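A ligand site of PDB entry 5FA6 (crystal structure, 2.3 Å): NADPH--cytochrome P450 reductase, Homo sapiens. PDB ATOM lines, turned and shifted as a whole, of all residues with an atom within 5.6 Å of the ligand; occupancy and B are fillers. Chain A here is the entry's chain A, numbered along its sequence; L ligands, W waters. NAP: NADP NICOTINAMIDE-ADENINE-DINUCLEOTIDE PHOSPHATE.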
ATOM      1  N   ARG A 239      33.664 -16.388  30.159  1.00  0.00           N
ATOM      2  CA  ARG A 239      33.346 -16.566  28.741  1.00  0.00           C
ATOM      3  C   ARG A 239      34.630 -16.877  27.989  1.00  0.00           C
ATOM      4  O   ARG A 239      35.725 -16.707  28.527  1.00  0.00           O
ATOM      5  CB  ARG A 239      32.748 -15.293  28.149  1.00  0.00           C
ATOM      6  CG  ARG A 239      31.547 -14.739  28.881  1.00  0.00           C
ATOM      7  CD  ARG A 239      30.745 -13.825  27.967  1.00  0.00           C
ATOM      8  NE  ARG A 239      31.467 -12.628  27.541  1.00  0.00           N
ATOM      9  CZ  ARG A 239      31.126 -11.908  26.479  1.00  0.00           C
ATOM     10  NH1 ARG A 239      30.080 -12.256  25.728  1.00  0.00           N
ATOM     11  NH2 ARG A 239      31.812 -10.811  26.183  1.00  0.00           N
ATOM     12  N   LEU A 241      36.385 -16.002  24.267  1.00  0.00           N
ATOM     13  CA  LEU A 241      36.387 -15.378  22.937  1.00  0.00           C
ATOM     14  C   LEU A 241      37.716 -15.761  22.269  1.00  0.00           C
ATOM     15  O   LEU A 241      38.782 -15.613  22.851  1.00  0.00           O
ATOM     16  CB  LEU A 241      36.185 -13.870  23.021  1.00  0.00           C
ATOM     17  CG  LEU A 241      34.775 -13.572  23.574  1.00  0.00           C
ATOM     18  CD1 LEU A 241      34.882 -13.423  25.095  1.00  0.00           C
ATOM     19  CD2 LEU A 241      34.196 -12.299  22.977  1.00  0.00           C
ATOM     20  N   VAL A 415      32.728 -16.023  19.740  1.00  0.00           N
ATOM     21  CA  VAL A 415      32.405 -16.165  21.143  1.00  0.00           C
ATOM     22  C   VAL A 415      31.812 -17.562  21.305  1.00  0.00           C
ATOM     23  O   VAL A 415      30.902 -17.952  20.557  1.00  0.00           O
ATOM     24  CB  VAL A 415      31.412 -15.059  21.608  1.00  0.00           C
ATOM     25  CG1 VAL A 415      30.114 -15.097  20.789  1.00  0.00           C
ATOM     26  CG2 VAL A 415      31.093 -15.220  23.101  1.00  0.00           C
ATOM     27  N   PRO A 474      30.102  -3.777  18.032  1.00  0.00           N
ATOM     28  CA  PRO A 474      30.489  -4.155  19.401  1.00  0.00           C
ATOM     29  C   PRO A 474      30.536  -5.683  19.548  1.00  0.00           C
ATOM     30  O   PRO A 474      29.870  -6.413  18.796  1.00  0.00           O
ATOM     31  CB  PRO A 474      29.425  -3.514  20.264  1.00  0.00           C
ATOM     32  CG  PRO A 474      28.195  -3.612  19.386  1.00  0.00           C
ATOM     33  CD  PRO A 474      28.716  -3.247  18.002  1.00  0.00           C
ATOM     34  N   GLY A 475      31.305  -6.152  20.521  1.00  0.00           N
ATOM     35  CA  GLY A 475      31.420  -7.589  20.734  1.00  0.00           C
ATOM     36  C   GLY A 475      32.057  -8.239  19.517  1.00  0.00           C
ATOM     37  O   GLY A 475      32.959  -7.688  18.905  1.00  0.00           O
ATOM     38  N   THR A 476      31.564  -9.414  19.147  1.00  0.00           N
ATOM     39  CA  THR A 476      32.117 -10.121  17.999  1.00  0.00           C
ATOM     40  C   THR A 476      31.785  -9.403  16.705  1.00  0.00           C
ATOM     41  O   THR A 476      32.296  -9.740  15.659  1.00  0.00           O
ATOM     42  CB  THR A 476      31.620 -11.581  17.939  1.00  0.00           C
ATOM     43  OG1 THR A 476      30.190 -11.623  17.972  1.00  0.00           O
ATOM     44  CG2 THR A 476      32.185 -12.365  19.092  1.00  0.00           C
ATOM     45  N   GLY A 477      30.931  -8.389  16.796  1.00  0.00           N
ATOM     46  CA  GLY A 477      30.571  -7.604  15.630  1.00  0.00           C
ATOM     47  C   GLY A 477      31.775  -6.840  15.081  1.00  0.00           C
ATOM     48  O   GLY A 477      31.721  -6.270  14.000  1.00  0.00           O
ATOM     49  N   GLY A 506      32.718  -1.820  21.142  1.00  0.00           N
ATOM     50  CA  GLY A 506      32.158  -1.864  22.480  1.00  0.00           C
ATOM     51  C   GLY A 506      32.318  -3.221  23.132  1.00  0.00           C
ATOM     52  O   GLY A 506      32.443  -4.234  22.449  1.00  0.00           O
ATOM     53  N   CYS A 507      32.344  -3.215  24.455  1.00  0.00           N
ATOM     54  CA  CYS A 507      32.436  -4.433  25.248  1.00  0.00           C
ATOM     55  C   CYS A 507      31.994  -4.100  26.665  1.00  0.00           C
ATOM     56  O   CYS A 507      31.651  -2.944  26.934  1.00  0.00           O
ATOM     57  CB  CYS A 507      33.858  -5.010  25.220  1.00  0.00           C
ATOM     58  SG  CYS A 507      35.133  -3.921  25.835  1.00  0.00           S
ATOM     59  N   ARG A 508      32.002  -5.079  27.549  1.00  0.00           N
ATOM     60  CA  ARG A 508      31.563  -4.901  28.926  1.00  0.00           C
ATOM     61  C   ARG A 508      32.554  -4.160  29.811  1.00  0.00           C
ATOM     62  O   ARG A 508      32.209  -3.181  30.479  1.00  0.00           O
ATOM     63  CB  ARG A 508      31.225  -6.266  29.539  1.00  0.00           C
ATOM     64  CG  ARG A 508      30.137  -7.001  28.759  1.00  0.00           C
ATOM     65  CD  ARG A 508      29.937  -8.444  29.221  1.00  0.00           C
ATOM     66  NE  ARG A 508      29.078  -9.179  28.291  1.00  0.00           N
ATOM     67  CZ  ARG A 508      28.477 -10.334  28.556  1.00  0.00           C
ATOM     68  NH1 ARG A 508      28.640 -10.911  29.736  1.00  0.00           N
ATOM     69  NH2 ARG A 508      27.712 -10.913  27.641  1.00  0.00           N
ATOM     70  N   ASP A 513      36.695  -8.305  28.130  1.00  0.00           N
ATOM     71  CA  ASP A 513      36.453  -8.699  26.750  1.00  0.00           C
ATOM     72  C   ASP A 513      36.776  -7.652  25.677  1.00  0.00           C
ATOM     73  O   ASP A 513      36.060  -7.537  24.683  1.00  0.00           O
ATOM     74  CB  ASP A 513      34.999  -9.152  26.589  1.00  0.00           C
ATOM     75  CG  ASP A 513      34.024  -8.227  27.261  1.00  0.00           C
ATOM     76  OD1 ASP A 513      34.307  -7.015  27.320  1.00  0.00           O
ATOM     77  OD2 ASP A 513      32.978  -8.703  27.730  1.00  0.00           O
ATOM     78  N   ALA A 535      32.960   1.793  23.745  1.00  0.00           N
ATOM     79  CA  ALA A 535      31.938   1.961  24.769  1.00  0.00           C
ATOM     80  C   ALA A 535      31.944   0.768  25.702  1.00  0.00           C
ATOM     81  O   ALA A 535      31.606  -0.354  25.296  1.00  0.00           O
ATOM     82  CB  ALA A 535      30.552   2.103  24.132  1.00  0.00           C
ATOM     83  N   PHE A 536      32.340   1.003  26.955  1.00  0.00           N
ATOM     84  CA  PHE A 536      32.346  -0.041  27.981  1.00  0.00           C
ATOM     85  C   PHE A 536      30.987   0.063  28.673  1.00  0.00           C
ATOM     86  O   PHE A 536      30.713   1.029  29.372  1.00  0.00           O
ATOM     87  CB  PHE A 536      33.475   0.210  28.992  1.00  0.00           C
ATOM     88  CG  PHE A 536      34.822   0.363  28.355  1.00  0.00           C
ATOM     89  CD1 PHE A 536      35.415  -0.703  27.677  1.00  0.00           C
ATOM     90  CD2 PHE A 536      35.492   1.589  28.388  1.00  0.00           C
ATOM     91  CE1 PHE A 536      36.639  -0.554  27.040  1.00  0.00           C
ATOM     92  CE2 PHE A 536      36.717   1.748  27.754  1.00  0.00           C
ATOM     93  CZ  PHE A 536      37.299   0.672  27.076  1.00  0.00           C
ATOM     94  N   SER A 537      30.154  -0.953  28.471  1.00  0.00           N
ATOM     95  CA  SER A 537      28.801  -0.973  29.023  1.00  0.00           C
ATOM     96  C   SER A 537      28.663  -1.263  30.522  1.00  0.00           C
ATOM     97  O   SER A 537      27.658  -0.902  31.125  1.00  0.00           O
ATOM     98  CB  SER A 537      27.935  -1.963  28.240  1.00  0.00           C
ATOM     99  OG  SER A 537      28.467  -3.280  28.280  1.00  0.00           O
ATOM    100  N   ARG A 538      29.662  -1.910  31.111  1.00  0.00           N
ATOM    101  CA  ARG A 538      29.576  -2.262  32.531  1.00  0.00           C
ATOM    102  C   ARG A 538      30.718  -1.752  33.418  1.00  0.00           C
ATOM    103  O   ARG A 538      31.136  -2.456  34.344  1.00  0.00           O
ATOM    104  CB  ARG A 538      29.457  -3.778  32.675  1.00  0.00           C
ATOM    105  CG  ARG A 538      28.348  -4.376  31.827  1.00  0.00           C
ATOM    106  CD  ARG A 538      28.205  -5.870  32.038  1.00  0.00           C
ATOM    107  NE  ARG A 538      27.252  -6.443  31.079  1.00  0.00           N
ATOM    108  CZ  ARG A 538      26.824  -7.711  31.095  1.00  0.00           C
ATOM    109  NH1 ARG A 538      27.257  -8.553  32.026  1.00  0.00           N
ATOM    110  NH2 ARG A 538      25.970  -8.133  30.169  1.00  0.00           N
ATOM    111  N   LYS A 543      24.328   1.786  31.483  1.00  0.00           N
ATOM    112  CA  LYS A 543      24.857   1.283  30.224  1.00  0.00           C
ATOM    113  C   LYS A 543      25.425   2.343  29.295  1.00  0.00           C
ATOM    114  O   LYS A 543      24.829   3.413  29.115  1.00  0.00           O
ATOM    115  CB  LYS A 543      23.754   0.531  29.465  1.00  0.00           C
ATOM    116  CG  LYS A 543      23.177  -0.667  30.199  1.00  0.00           C
ATOM    117  CD  LYS A 543      24.206  -1.772  30.366  1.00  0.00           C
ATOM    118  CE  LYS A 543      23.567  -3.014  30.983  1.00  0.00           C
ATOM    119  NZ  LYS A 543      24.556  -4.108  31.155  1.00  0.00           N
ATOM    120  N   VAL A 544      26.577   2.052  28.706  1.00  0.00           N
ATOM    121  CA  VAL A 544      27.201   2.951  27.742  1.00  0.00           C
ATOM    122  C   VAL A 544      27.454   2.091  26.507  1.00  0.00           C
ATOM    123  O   VAL A 544      28.248   1.156  26.546  1.00  0.00           O
ATOM    124  CB  VAL A 544      28.537   3.528  28.238  1.00  0.00           C
ATOM    125  CG1 VAL A 544      29.229   4.278  27.096  1.00  0.00           C
ATOM    126  CG2 VAL A 544      28.284   4.473  29.402  1.00  0.00           C
ATOM    127  N   TYR A 545      26.761   2.411  25.422  1.00  0.00           N
ATOM    128  CA  TYR A 545      26.873   1.659  24.174  1.00  0.00           C
ATOM    129  C   TYR A 545      27.445   2.495  23.051  1.00  0.00           C
ATOM    130  O   TYR A 545      27.723   3.689  23.204  1.00  0.00           O
ATOM    131  CB  TYR A 545      25.518   1.120  23.762  1.00  0.00           C
ATOM    132  CG  TYR A 545      24.843   0.201  24.767  1.00  0.00           C
ATOM    133  CD1 TYR A 545      25.609  -0.601  25.630  1.00  0.00           C
ATOM    134  CD2 TYR A 545      23.460   0.077  24.814  1.00  0.00           C
ATOM    135  CE1 TYR A 545      25.001  -1.513  26.499  1.00  0.00           C
ATOM    136  CE2 TYR A 545      22.832  -0.845  25.685  1.00  0.00           C
ATOM    137  CZ  TYR A 545      23.612  -1.631  26.528  1.00  0.00           C
ATOM    138  OH  TYR A 545      23.037  -2.556  27.362  1.00  0.00           O
ATOM    139  N   VAL A 546      27.610   1.859  21.892  1.00  0.00           N
ATOM    140  CA  VAL A 546      28.147   2.498  20.703  1.00  0.00           C
ATOM    141  C   VAL A 546      27.242   3.619  20.190  1.00  0.00           C
ATOM    142  O   VAL A 546      27.730   4.644  19.728  1.00  0.00           O
ATOM    143  CB  VAL A 546      28.395   1.464  19.554  1.00  0.00           C
ATOM    144  CG1 VAL A 546      29.540   0.537  19.934  1.00  0.00           C
ATOM    145  CG2 VAL A 546      27.108   0.631  19.298  1.00  0.00           C
ATOM    146  N   GLN A 547      25.919   3.430  20.265  1.00  0.00           N
ATOM    147  CA  GLN A 547      25.015   4.467  19.789  1.00  0.00           C
ATOM    148  C   GLN A 547      25.085   5.741  20.635  1.00  0.00           C
ATOM    149  O   GLN A 547      24.602   6.793  20.223  1.00  0.00           O
ATOM    150  CB  GLN A 547      23.554   3.976  19.716  1.00  0.00           C
ATOM    151  CG  GLN A 547      22.929   3.488  21.012  1.00  0.00           C
ATOM    152  CD  GLN A 547      23.194   2.013  21.280  1.00  0.00           C
ATOM    153  OE1 GLN A 547      24.168   1.424  20.741  1.00  0.00           O
ATOM    154  NE2 GLN A 547      22.338   1.395  22.097  1.00  0.00           N
ATOM    155  N   ASP A 572      25.067  -7.994  16.859  1.00  0.00           N
ATOM    156  CA  ASP A 572      23.705  -8.341  17.317  1.00  0.00           C
ATOM    157  C   ASP A 572      22.611  -7.638  16.501  1.00  0.00           C
ATOM    158  O   ASP A 572      22.546  -6.403  16.458  1.00  0.00           O
ATOM    159  CB  ASP A 572      23.557  -7.960  18.789  1.00  0.00           C
ATOM    160  CG  ASP A 572      22.164  -8.257  19.327  1.00  0.00           C
ATOM    161  OD1 ASP A 572      21.768  -9.433  19.277  1.00  0.00           O
ATOM    162  OD2 ASP A 572      21.479  -7.334  19.809  1.00  0.00           O
ATOM    163  N   ASN A 575      18.768  -5.940  19.036  1.00  0.00           N
ATOM    164  CA  ASN A 575      18.603  -4.591  19.591  1.00  0.00           C
ATOM    165  C   ASN A 575      19.640  -3.590  19.089  1.00  0.00           C
ATOM    166  O   ASN A 575      19.297  -2.488  18.622  1.00  0.00           O
ATOM    167  CB  ASN A 575      18.644  -4.639  21.120  1.00  0.00           C
ATOM    168  CG  ASN A 575      17.523  -5.492  21.704  1.00  0.00           C
ATOM    169  OD1 ASN A 575      16.355  -5.100  21.666  1.00  0.00           O
ATOM    170  ND2 ASN A 575      17.871  -6.644  22.263  1.00  0.00           N
ATOM    171  N   MET A 576      20.912  -3.970  19.168  1.00  0.00           N
ATOM    172  CA  MET A 576      21.996  -3.094  18.754  1.00  0.00           C
ATOM    173  C   MET A 576      21.796  -2.440  17.370  1.00  0.00           C
ATOM    174  O   MET A 576      21.752  -1.215  17.252  1.00  0.00           O
ATOM    175  CB  MET A 576      23.320  -3.869  18.808  1.00  0.00           C
ATOM    176  CG  MET A 576      24.550  -3.048  18.510  1.00  0.00           C
ATOM    177  SD  MET A 576      24.804  -2.768  16.747  1.00  0.00           S
ATOM    178  CE  MET A 576      25.463  -4.375  16.276  1.00  0.00           C
ATOM    179  N   ASP A 579      18.930  -0.007  17.472  1.00  0.00           N
ATOM    180  CA  ASP A 579      19.212   1.189  18.256  1.00  0.00           C
ATOM    181  C   ASP A 579      20.188   2.110  17.484  1.00  0.00           C
ATOM    182  O   ASP A 579      20.058   3.329  17.507  1.00  0.00           O
ATOM    183  CB  ASP A 579      19.819   0.825  19.634  1.00  0.00           C
ATOM    184  CG  ASP A 579      18.822   0.136  20.575  1.00  0.00           C
ATOM    185  OD1 ASP A 579      17.632   0.519  20.605  1.00  0.00           O
ATOM    186  OD2 ASP A 579      19.228  -0.794  21.321  1.00  0.00           O
ATOM    187  N   VAL A 580      21.154   1.495  16.797  1.00  0.00           N
ATOM    188  CA  VAL A 580      22.153   2.246  16.061  1.00  0.00           C
ATOM    189  C   VAL A 580      21.574   2.934  14.847  1.00  0.00           C
ATOM    190  O   VAL A 580      22.050   3.981  14.418  1.00  0.00           O
ATOM    191  CB  VAL A 580      23.309   1.308  15.596  1.00  0.00           C
ATOM    192  CG1 VAL A 580      24.169   2.012  14.534  1.00  0.00           C
ATOM    193  CG2 VAL A 580      24.151   0.897  16.806  1.00  0.00           C
HETATM  194  PA  NAP L   1      28.118  -9.026  23.752  1.00  0.00           P
HETATM  195  O1A NAP L   1      29.367  -9.335  24.481  1.00  0.00           O
HETATM  196  O2A NAP L   1      26.858  -9.656  24.220  1.00  0.00           O
HETATM  197  O5B NAP L   1      27.914  -7.437  23.679  1.00  0.00           O
HETATM  198  C5B NAP L   1      29.001  -6.615  23.236  1.00  0.00           C
HETATM  199  C4B NAP L   1      28.775  -5.167  23.688  1.00  0.00           C
HETATM  200  O4B NAP L   1      27.523  -4.708  23.151  1.00  0.00           O
HETATM  201  C3B NAP L   1      28.644  -5.105  25.203  1.00  0.00           C
HETATM  202  O3B NAP L   1      29.206  -3.874  25.681  1.00  0.00           O
HETATM  203  C2B NAP L   1      27.143  -5.109  25.398  1.00  0.00           C
HETATM  204  O2B NAP L   1      26.817  -4.491  26.650  1.00  0.00           O
HETATM  205  C1B NAP L   1      26.800  -4.159  24.271  1.00  0.00           C
HETATM  206  N9A NAP L   1      25.345  -4.041  23.994  1.00  0.00           N
HETATM  207  C8A NAP L   1      24.366  -4.813  24.456  1.00  0.00           C
HETATM  208  N7A NAP L   1      23.222  -4.386  23.933  1.00  0.00           N
HETATM  209  C5A NAP L   1      23.496  -3.360  23.139  1.00  0.00           C
HETATM  210  C6A NAP L   1      22.707  -2.590  22.381  1.00  0.00           C
HETATM  211  N6A NAP L   1      21.402  -2.838  22.442  1.00  0.00           N
HETATM  212  N1A NAP L   1      23.196  -1.606  21.612  1.00  0.00           N
HETATM  213  C2A NAP L   1      24.579  -1.381  21.609  1.00  0.00           C
HETATM  214  N3A NAP L   1      25.381  -2.198  22.414  1.00  0.00           N
HETATM  215  C4A NAP L   1      24.814  -3.149  23.161  1.00  0.00           C
HETATM  216  O3  NAP L   1      28.327  -9.406  22.198  1.00  0.00           O
HETATM  217  PN  NAP L   1      28.918 -10.760  21.568  1.00  0.00           P
HETATM  218  O1N NAP L   1      29.779 -10.423  20.407  1.00  0.00           O
HETATM  219  O2N NAP L   1      29.488 -11.579  22.664  1.00  0.00           O
HETATM  220  O5D NAP L   1      27.588 -11.485  21.043  1.00  0.00           O
HETATM  221  P2B NAP L   1      25.965  -5.248  27.779  1.00  0.00           P
HETATM  222  O1X NAP L   1      26.709  -4.958  29.018  1.00  0.00           O
HETATM  223  O2X NAP L   1      24.617  -4.632  27.701  1.00  0.00           O
HETATM  224  O3X NAP L   1      26.014  -6.674  27.361  1.00  0.00           O
HETATM  225  O   HOH W   1      29.264  -1.594  24.479  1.00  0.00           O
HETATM  226  O   HOH W   2      25.442 -11.536  18.387  1.00  0.00           O
HETATM  227  O   HOH W   3      18.948  -3.826  24.144  1.00  0.00           O
HETATM  228  O   HOH W   4      25.483  -6.053  21.258  1.00  0.00           O
HETATM  229  O   HOH W   5      27.799  -0.763  22.218  1.00  0.00           O
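N of Ser 537 is in hydrogen-bond range of O of Cys 507, 2.9 Å away.
N of Ser 537 sits close to O of Val 544 (3.4 Å).
O of Arg 508 is in hydrogen-bond range of N of Arg 538 (2.9 Å).
The guanidinium group (NH2) of Arg 239 is in salt-bridge range of the side-chain carboxylate (OD2) of Asp 513 (2.9 Å).
The backbone carbonyl oxygen (O) of Gly 506 sits at hydrogen-bond distance from the backbone NH (N) of Gly 475, at 2.9 Å.
The backbone NH (N) of Met 576 is in hydrogen-bond range of the side-chain carboxylate (OD2) of Asp 572 (3.5 Å).
The backbone NH of Asn 575 is in hydrogen-bond range of the side-chain carboxylate of Asp 572 (3.1 Å).
NE of Arg 508 lies within salt-bridge range of OD2 of Asp 513, at 3.97 Å.
N of Thr 476 sits at hydrogen-bond distance from O1N of the ligand, at 2.4 Å.
An oxygen (O1N) of the ligand lies within hydrogen-bond range of the side-chain hydroxyl of Thr 476, 2.7 Å away.
The side-chain hydroxyl (OG) of Ser 537 sits at hydrogen-bond distance from an oxygen (O1X) of the ligand (2.5 Å).
The guanidinium group of Arg 538 is in salt-bridge range of an oxygen (O1X) of the ligand, 2.6 Å away.
The side-chain hydroxyl of Tyr 545 lies within hydrogen-bond range of an oxygen (O2X) of the ligand.
O3B of the ligand lies close to N of Cys 507, 3.4 Å away.
The backbone carbonyl oxygen (O) of Cys 507 sits at hydrogen-bond distance from an oxygen (O3B) of the ligand (2.9 Å).
The side-chain amide nitrogen (NE2) of Gln 547 lies within hydrogen-bond range of a nitrogen (N1A) of the ligand, at 3.2 Å.
NZ of Lys 543 is in salt-bridge range of O1X of the ligand, at 3.2 Å.
OD2 of Asp 579 is in hydrogen-bond range of N6A of the ligand (3.2 Å).
The guanidinium group (NH1) of Arg 239 lies within salt-bridge range of an oxygen (O2N) of the ligand (3.2 Å).
NH2 of Arg 508 is in salt-bridge range of O2A of the ligand, at 3.7 Å.
N of Met 576 sits close to N6A of the ligand.
Pro 474 touches the ligand (CB to O4B, 3.7 Å).
C of Gly 475 touches O1N of the ligand, 3.3 Å away.
O of Gly 506 touches C4B of the ligand, 3.98 Å away.
Val 546 touches the ligand.
Asn 575 touches the ligand (CB to N6A, 3.5 Å).
Hydrophobic or aromatic side chains that line the ligand: Pro 474, Tyr 545, Val 546 and Met 576.
16 residues have an atom within 4 Å of the ligand: Arg 239, Pro 474, Gly 475, Thr 476, Gly 506, Cys 507, Arg 508, Ser 537, Arg 538, Lys 543, Tyr 545, Val 546, Gln 547, Asn 575, Met 576 and Asp 579.
The nearest printed residue that does not touch the ligand is Val 415 (4.003 Å).
Water W1 lies within hydrogen-bond range of O3B of the ligand (2.6 Å), O of Ala 535 (2.8 Å) and N of Cys 507 (3.5 Å).
Water W5 lies within hydrogen-bond range of the backbone NH of Val 546 (2.6 Å) and a nitrogen (N3A) of the ligand (2.8 Å).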
